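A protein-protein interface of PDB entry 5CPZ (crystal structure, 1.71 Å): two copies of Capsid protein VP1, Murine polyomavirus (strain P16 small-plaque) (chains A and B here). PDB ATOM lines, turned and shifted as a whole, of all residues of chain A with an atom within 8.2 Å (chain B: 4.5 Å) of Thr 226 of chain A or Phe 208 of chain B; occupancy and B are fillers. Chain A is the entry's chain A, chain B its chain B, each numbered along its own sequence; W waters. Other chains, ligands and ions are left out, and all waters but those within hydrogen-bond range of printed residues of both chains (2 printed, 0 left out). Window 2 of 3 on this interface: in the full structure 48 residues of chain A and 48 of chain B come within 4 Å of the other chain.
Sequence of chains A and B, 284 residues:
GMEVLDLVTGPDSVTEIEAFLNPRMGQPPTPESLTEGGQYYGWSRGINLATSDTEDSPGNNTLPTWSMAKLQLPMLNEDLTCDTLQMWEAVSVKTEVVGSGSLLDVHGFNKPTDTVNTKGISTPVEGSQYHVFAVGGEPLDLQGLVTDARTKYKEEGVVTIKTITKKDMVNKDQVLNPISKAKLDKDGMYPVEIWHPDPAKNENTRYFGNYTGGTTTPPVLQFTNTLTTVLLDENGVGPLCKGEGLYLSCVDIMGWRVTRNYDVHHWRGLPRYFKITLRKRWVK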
ATOM      1  N   LYS A  94       5.037 -19.840  -1.148  1.00  0.00           N
ATOM      2  CA  LYS A  94       4.376 -20.083   0.119  1.00  0.00           C
ATOM      3  C   LYS A  94       3.439 -18.916   0.338  1.00  0.00           C
ATOM      4  O   LYS A  94       3.862 -17.756   0.346  1.00  0.00           O
ATOM      5  CB  LYS A  94       5.398 -20.210   1.248  1.00  0.00           C
ATOM      6  CG  LYS A  94       6.316 -21.405   1.055  1.00  0.00           C
ATOM      7  CD  LYS A  94       7.415 -21.459   2.098  1.00  0.00           C
ATOM      8  CE  LYS A  94       6.965 -22.242   3.316  1.00  0.00           C
ATOM      9  NZ  LYS A  94       8.114 -22.530   4.219  1.00  0.00           N
ATOM     10  N   THR A  95       2.151 -19.214   0.456  1.00  0.00           N
ATOM     11  CA  THR A  95       1.165 -18.163   0.615  1.00  0.00           C
ATOM     12  C   THR A  95       0.253 -18.470   1.797  1.00  0.00           C
ATOM     13  O   THR A  95      -0.049 -19.637   2.073  1.00  0.00           O
ATOM     14  CB  THR A  95       0.382 -17.886  -0.691  1.00  0.00           C
ATOM     15  OG1 THR A  95      -0.479 -16.762  -0.493  1.00  0.00           O
ATOM     16  CG2 THR A  95      -0.462 -19.096  -1.126  1.00  0.00           C
ATOM     17  N   GLU A  96      -0.152 -17.415   2.496  1.00  0.00           N
ATOM     18  CA  GLU A  96      -0.934 -17.543   3.720  1.00  0.00           C
ATOM     19  C   GLU A  96      -1.895 -16.368   3.858  1.00  0.00           C
ATOM     20  O   GLU A  96      -1.532 -15.229   3.571  1.00  0.00           O
ATOM     21  CB  GLU A  96       0.019 -17.597   4.920  1.00  0.00           C
ATOM     22  CG  GLU A  96      -0.640 -17.838   6.268  1.00  0.00           C
ATOM     23  CD  GLU A  96       0.370 -18.226   7.332  1.00  0.00           C
ATOM     24  OE1 GLU A  96       1.308 -18.988   7.025  1.00  0.00           O
ATOM     25  OE2 GLU A  96       0.226 -17.772   8.474  1.00  0.00           O
ATOM     26  N   GLN A 222      -7.434 -22.281   6.962  1.00  0.00           N
ATOM     27  CA  GLN A 222      -6.246 -22.921   7.506  1.00  0.00           C
ATOM     28  C   GLN A 222      -5.053 -22.034   7.206  1.00  0.00           C
ATOM     29  O   GLN A 222      -5.059 -21.283   6.223  1.00  0.00           O
ATOM     30  CB  GLN A 222      -6.027 -24.312   6.898  1.00  0.00           C
ATOM     31  CG  GLN A 222      -7.135 -25.317   7.182  1.00  0.00           C
ATOM     32  CD  GLN A 222      -8.243 -25.289   6.145  1.00  0.00           C
ATOM     33  OE1 GLN A 222      -9.424 -25.231   6.486  1.00  0.00           O
ATOM     34  NE2 GLN A 222      -7.867 -25.331   4.870  1.00  0.00           N
ATOM     35  N   PHE A 223      -4.041 -22.112   8.060  1.00  0.00           N
ATOM     36  CA  PHE A 223      -2.816 -21.328   7.883  1.00  0.00           C
ATOM     37  C   PHE A 223      -1.637 -22.063   8.492  1.00  0.00           C
ATOM     38  O   PHE A 223      -1.733 -22.623   9.584  1.00  0.00           O
ATOM     39  CB  PHE A 223      -2.952 -19.897   8.449  1.00  0.00           C
ATOM     40  CG  PHE A 223      -3.451 -19.829   9.872  1.00  0.00           C
ATOM     41  CD1 PHE A 223      -4.815 -19.922  10.157  1.00  0.00           C
ATOM     42  CD2 PHE A 223      -2.561 -19.632  10.929  1.00  0.00           C
ATOM     43  CE1 PHE A 223      -5.277 -19.850  11.469  1.00  0.00           C
ATOM     44  CE2 PHE A 223      -3.019 -19.557  12.240  1.00  0.00           C
ATOM     45  CZ  PHE A 223      -4.380 -19.666  12.509  1.00  0.00           C
ATOM     46  N   THR A 224      -0.533 -22.090   7.751  1.00  0.00           N
ATOM     47  CA  THR A 224       0.691 -22.728   8.201  1.00  0.00           C
ATOM     48  C   THR A 224       1.851 -22.160   7.399  1.00  0.00           C
ATOM     49  O   THR A 224       1.660 -21.719   6.266  1.00  0.00           O
ATOM     50  CB  THR A 224       0.646 -24.267   8.034  1.00  0.00           C
ATOM     51  OG1 THR A 224       1.871 -24.841   8.495  1.00  0.00           O
ATOM     52  CG2 THR A 224       0.419 -24.678   6.579  1.00  0.00           C
ATOM     53  N   ASN A 225       3.044 -22.165   7.985  1.00  0.00           N
ATOM     54  CA  ASN A 225       4.244 -21.756   7.254  1.00  0.00           C
ATOM     55  C   ASN A 225       5.005 -22.937   6.648  1.00  0.00           C
ATOM     56  O   ASN A 225       6.167 -22.800   6.248  1.00  0.00           O
ATOM     57  CB  ASN A 225       5.159 -20.877   8.136  1.00  0.00           C
ATOM     58  CG  ASN A 225       5.748 -21.623   9.327  1.00  0.00           C
ATOM     59  OD1 ASN A 225       5.246 -22.672   9.747  1.00  0.00           O
ATOM     60  ND2 ASN A 225       6.834 -21.076   9.879  1.00  0.00           N
ATOM     61  N   THR A 226       4.342 -24.093   6.571  1.00  0.00           N
ATOM     62  CA  THR A 226       4.992 -25.342   6.143  1.00  0.00           C
ATOM     63  C   THR A 226       4.522 -25.855   4.774  1.00  0.00           C
ATOM     64  O   THR A 226       4.967 -26.923   4.335  1.00  0.00           O
ATOM     65  CB  THR A 226       4.752 -26.474   7.163  1.00  0.00           C
ATOM     66  OG1 THR A 226       3.349 -26.791   7.200  1.00  0.00           O
ATOM     67  CG2 THR A 226       5.231 -26.068   8.559  1.00  0.00           C
ATOM     68  N   LEU A 227       3.639 -25.100   4.120  1.00  0.00           N
ATOM     69  CA  LEU A 227       3.037 -25.522   2.854  1.00  0.00           C
ATOM     70  C   LEU A 227       3.574 -24.728   1.662  1.00  0.00           C
ATOM     71  O   LEU A 227       3.481 -23.500   1.622  1.00  0.00           O
ATOM     72  CB  LEU A 227       1.505 -25.416   2.940  1.00  0.00           C
ATOM     73  CG  LEU A 227       0.620 -25.821   1.752  1.00  0.00           C
ATOM     74  CD1 LEU A 227       0.756 -27.302   1.426  1.00  0.00           C
ATOM     75  CD2 LEU A 227      -0.835 -25.470   2.035  1.00  0.00           C
ATOM     76  N   THR A 228       4.122 -25.451   0.693  1.00  0.00           N
ATOM     77  CA  THR A 228       4.669 -24.859  -0.515  1.00  0.00           C
ATOM     78  C   THR A 228       3.813 -25.246  -1.718  1.00  0.00           C
ATOM     79  O   THR A 228       3.519 -26.429  -1.921  1.00  0.00           O
ATOM     80  CB  THR A 228       6.114 -25.342  -0.719  1.00  0.00           C
ATOM     81  OG1 THR A 228       6.927 -24.828   0.341  1.00  0.00           O
ATOM     82  CG2 THR A 228       6.677 -24.889  -2.068  1.00  0.00           C
ATOM     83  N   THR A 229       3.423 -24.242  -2.501  1.00  0.00           N
ATOM     84  CA  THR A 229       2.694 -24.451  -3.751  1.00  0.00           C
ATOM     85  C   THR A 229       3.689 -24.428  -4.913  1.00  0.00           C
ATOM     86  O   THR A 229       4.328 -23.400  -5.152  1.00  0.00           O
ATOM     87  CB  THR A 229       1.632 -23.344  -3.961  1.00  0.00           C
ATOM     88  OG1 THR A 229       0.750 -23.279  -2.830  1.00  0.00           O
ATOM     89  CG2 THR A 229       0.812 -23.595  -5.222  1.00  0.00           C
ATOM     90  N   HIS B 131      -7.701 -23.528  16.469  1.00  0.00           N
ATOM     91  CA  HIS B 131      -6.674 -24.472  16.901  1.00  0.00           C
ATOM     92  C   HIS B 131      -5.370 -24.104  16.240  1.00  0.00           C
ATOM     93  O   HIS B 131      -5.274 -24.136  15.015  1.00  0.00           O
ATOM     94  CB  HIS B 131      -7.073 -25.901  16.533  1.00  0.00           C
ATOM     95  CG  HIS B 131      -8.290 -26.381  17.259  1.00  0.00           C
ATOM     96  ND1 HIS B 131      -8.256 -26.761  18.583  1.00  0.00           N
ATOM     97  CD2 HIS B 131      -9.580 -26.500  16.865  1.00  0.00           C
ATOM     98  CE1 HIS B 131      -9.469 -27.120  18.965  1.00  0.00           C
ATOM     99  NE2 HIS B 131     -10.291 -26.968  17.944  1.00  0.00           N
ATOM    100  N   VAL B 132      -4.384 -23.712  17.046  1.00  0.00           N
ATOM    101  CA  VAL B 132      -3.037 -23.447  16.530  1.00  0.00           C
ATOM    102  C   VAL B 132      -2.007 -24.066  17.456  1.00  0.00           C
ATOM    103  O   VAL B 132      -2.154 -24.010  18.674  1.00  0.00           O
ATOM    104  CB  VAL B 132      -2.713 -21.938  16.405  1.00  0.00           C
ATOM    105  CG1 VAL B 132      -1.485 -21.744  15.518  1.00  0.00           C
ATOM    106  CG2 VAL B 132      -3.890 -21.157  15.839  1.00  0.00           C
ATOM    107  N   PHE B 133      -0.973 -24.670  16.884  1.00  0.00           N
ATOM    108  CA  PHE B 133       0.204 -25.007  17.679  1.00  0.00           C
ATOM    109  C   PHE B 133       1.474 -24.634  16.926  1.00  0.00           C
ATOM    110  O   PHE B 133       1.462 -24.505  15.700  1.00  0.00           O
ATOM    111  CB  PHE B 133       0.204 -26.477  18.135  1.00  0.00           C
ATOM    112  CG  PHE B 133       0.542 -27.471  17.051  1.00  0.00           C
ATOM    113  CD1 PHE B 133      -0.448 -27.967  16.208  1.00  0.00           C
ATOM    114  CD2 PHE B 133       1.850 -27.929  16.888  1.00  0.00           C
ATOM    115  CE1 PHE B 133      -0.141 -28.895  15.221  1.00  0.00           C
ATOM    116  CE2 PHE B 133       2.163 -28.856  15.900  1.00  0.00           C
ATOM    117  CZ  PHE B 133       1.163 -29.338  15.066  1.00  0.00           C
ATOM    118  N   ARG B 206       7.919 -23.828  13.337  1.00  0.00           N
ATOM    119  CA  ARG B 206       6.831 -24.327  12.483  1.00  0.00           C
ATOM    120  C   ARG B 206       5.507 -24.127  13.203  1.00  0.00           C
ATOM    121  O   ARG B 206       5.378 -24.492  14.377  1.00  0.00           O
ATOM    122  CB  ARG B 206       7.020 -25.816  12.146  1.00  0.00           C
ATOM    123  CG  ARG B 206       8.434 -26.242  11.763  1.00  0.00           C
ATOM    124  CD  ARG B 206       8.964 -25.546  10.510  1.00  0.00           C
ATOM    125  NE  ARG B 206      10.275 -26.100  10.191  1.00  0.00           N
ATOM    126  CZ  ARG B 206      11.434 -25.449  10.240  1.00  0.00           C
ATOM    127  NH1 ARG B 206      11.496 -24.154  10.537  1.00  0.00           N
ATOM    128  NH2 ARG B 206      12.544 -26.107   9.953  1.00  0.00           N
ATOM    129  N   TYR B 207       4.527 -23.536  12.519  1.00  0.00           N
ATOM    130  CA  TYR B 207       3.190 -23.382  13.099  1.00  0.00           C
ATOM    131  C   TYR B 207       2.101 -23.922  12.170  1.00  0.00           C
ATOM    132  O   TYR B 207       2.273 -23.966  10.955  1.00  0.00           O
ATOM    133  CB  TYR B 207       2.911 -21.927  13.513  1.00  0.00           C
ATOM    134  CG  TYR B 207       2.907 -20.928  12.376  1.00  0.00           C
ATOM    135  CD1 TYR B 207       1.770 -20.743  11.579  1.00  0.00           C
ATOM    136  CD2 TYR B 207       4.032 -20.154  12.109  1.00  0.00           C
ATOM    137  CE1 TYR B 207       1.768 -19.827  10.536  1.00  0.00           C
ATOM    138  CE2 TYR B 207       4.035 -19.231  11.082  1.00  0.00           C
ATOM    139  CZ  TYR B 207       2.910 -19.076  10.297  1.00  0.00           C
ATOM    140  OH  TYR B 207       2.937 -18.156   9.287  1.00  0.00           O
ATOM    141  N   PHE B 208       0.982 -24.330  12.769  1.00  0.00           N
ATOM    142  CA  PHE B 208      -0.104 -24.995  12.056  1.00  0.00           C
ATOM    143  C   PHE B 208      -1.397 -24.533  12.706  1.00  0.00           C
ATOM    144  O   PHE B 208      -1.600 -24.754  13.900  1.00  0.00           O
ATOM    145  CB  PHE B 208       0.011 -26.525  12.178  1.00  0.00           C
ATOM    146  CG  PHE B 208       1.391 -27.071  11.912  1.00  0.00           C
ATOM    147  CD1 PHE B 208       2.363 -27.078  12.913  1.00  0.00           C
ATOM    148  CD2 PHE B 208       1.711 -27.601  10.670  1.00  0.00           C
ATOM    149  CE1 PHE B 208       3.636 -27.586  12.667  1.00  0.00           C
ATOM    150  CE2 PHE B 208       2.974 -28.120  10.422  1.00  0.00           C
ATOM    151  CZ  PHE B 208       3.939 -28.110  11.420  1.00  0.00           C
ATOM    152  N   GLY B 209      -2.262 -23.882  11.933  1.00  0.00           N
ATOM    153  CA  GLY B 209      -3.485 -23.311  12.493  1.00  0.00           C
ATOM    154  C   GLY B 209      -4.722 -23.567  11.659  1.00  0.00           C
ATOM    155  O   GLY B 209      -4.644 -23.774  10.444  1.00  0.00           O
ATOM    156  N   THR B 229       3.977 -35.225  13.590  1.00  0.00           N
ATOM    157  CA  THR B 229       4.216 -34.044  12.757  1.00  0.00           C
ATOM    158  C   THR B 229       5.721 -33.844  12.558  1.00  0.00           C
ATOM    159  O   THR B 229       6.437 -33.537  13.516  1.00  0.00           O
ATOM    160  CB  THR B 229       3.618 -32.777  13.404  1.00  0.00           C
ATOM    161  OG1 THR B 229       2.228 -32.982  13.687  1.00  0.00           O
ATOM    162  CG2 THR B 229       3.769 -31.568  12.489  1.00  0.00           C
ATOM    163  N   LEU B 231       8.978 -31.842  11.625  1.00  0.00           N
ATOM    164  CA  LEU B 231       9.291 -30.415  11.760  1.00  0.00           C
ATOM    165  C   LEU B 231      10.446 -29.977  10.866  1.00  0.00           C
ATOM    166  O   LEU B 231      10.833 -28.803  10.867  1.00  0.00           O
ATOM    167  CB  LEU B 231       9.585 -30.060  13.229  1.00  0.00           C
ATOM    168  CG  LEU B 231       8.436 -30.286  14.219  1.00  0.00           C
ATOM    169  CD1 LEU B 231       8.926 -30.203  15.664  1.00  0.00           C
ATOM    170  CD2 LEU B 231       7.313 -29.282  13.977  1.00  0.00           C
HETATM  171  O   HOH W   1      -2.913 -25.734   9.031  1.00  0.00           O
HETATM  172  O   HOH W   2      10.002 -22.023   9.339  1.00  0.00           O
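O of Asn 225 of chain A is in hydrogen-bond range of NZ of Lys 94 of chain A.
The side-chain hydroxyl of Thr 224 of chain A sits at hydrogen-bond distance from the side-chain hydroxyl of Thr 226 of chain A, at 2.8 Å.
The backbone carbonyl oxygen (O) of Phe 133 of chain B sits at hydrogen-bond distance from the backbone NH (N) of Phe 208 of chain B.
The guanidinium group (NE) of Arg 206 of chain B sits at hydrogen-bond distance from the backbone carbonyl oxygen (O) of Leu 231 of chain B, 2.8 Å away.
1 position is printed for both chains.
Of the 10 pairs that touch across the chains among the printed residues, none has its exchanged pair printed and touching as well.
Gly 209 of chain B touches Gln 222 of chain A.
CZ of Phe 223 of chain A touches CG2 of Val 132 of chain B, at 3.7 Å.
C of Phe 208 of chain B touches O of Phe 223 of chain A (3.7 Å).
CD2 of Phe 208 of chain B touches OG1 of Thr 224 of chain A (3.5 Å).
Asn 225 of chain A touches Arg 206 of chain B (OD1 to CA, 3.6 Å).
Thr 226 of chain A touches Phe 208 of chain B (OG1 to CE2, 3.5 Å).
Printed residues of chain B that touch a printed residue of chain A: Val 132, Arg 206, Tyr 207, Phe 208 and Gly 209.
Hydrophobic or aromatic side chains of chain B within 4 Å of the printed part of chain A: Val 132, Tyr 207 and Phe 208.
Among the printed residues, 10 pairs touch across the chains.
Among the printed residues, no Asp or Glu carboxylate lies within 4 Å of a Lys or Arg side-chain nitrogen of the other chain.
The side-chain amide oxygen (OD1) of Asn 225 of chain A lies within hydrogen-bond range of the backbone NH (N) of Tyr 207 of chain B (3.0 Å).
OE2 of Glu 96 of chain A lies within hydrogen-bond range of OH of Tyr 207 of chain B (2.9 Å).
The side-chain hydroxyl of Thr 224 of chain A sits at hydrogen-bond distance from the backbone carbonyl oxygen of Tyr 207 of chain B (2.6 Å).
O of Phe 223 of chain A lies within hydrogen-bond range of N of Gly 209 of chain B (2.7 Å).
Water W2 bridges the guanidinium group of Arg 206 of chain B (2.9 Å) and the side-chain amide nitrogen of Asn 225 of chain A (3.4 Å).
Water W1 lies within hydrogen-bond range of O of Gly 209 of chain B and O of Phe 223 of chain A.
Printed residues of chain B within 4 Å of Phe 223 of chain A: Val 132 (3.7 Å), Phe 208 (3.7 Å) and Gly 209 (2.7 Å).
Printed residues of chain B within 4 Å of Thr 226 of chain A: Phe 208 (3.5 Å).
Of the printed residues of chain A, Val 132 of chain B touches Phe 223.
Of the printed residues of chain A, Tyr 207 of chain B touches Glu 96, Thr 224 and Asn 225.
Of the printed residues of chain A, Phe 208 of chain B touches Phe 223, Thr 224 and Thr 226.
Printed residues of chain A within 4 Å of Gly 209 of chain B: Gln 222 (3.5 Å) and Phe 223 (2.7 Å).
The nearest printed residue of chain B that does not touch Thr 226 of chain A is Arg 206 of chain B (4.02 Å).
The nearest residue of chain A that does not touch Phe 208 of chain B is Asn 225 of chain A (5.5 Å).
The nearest printed residue of chain B that does not touch Asn 225 of chain A is Phe 208 of chain B (5.5 Å).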
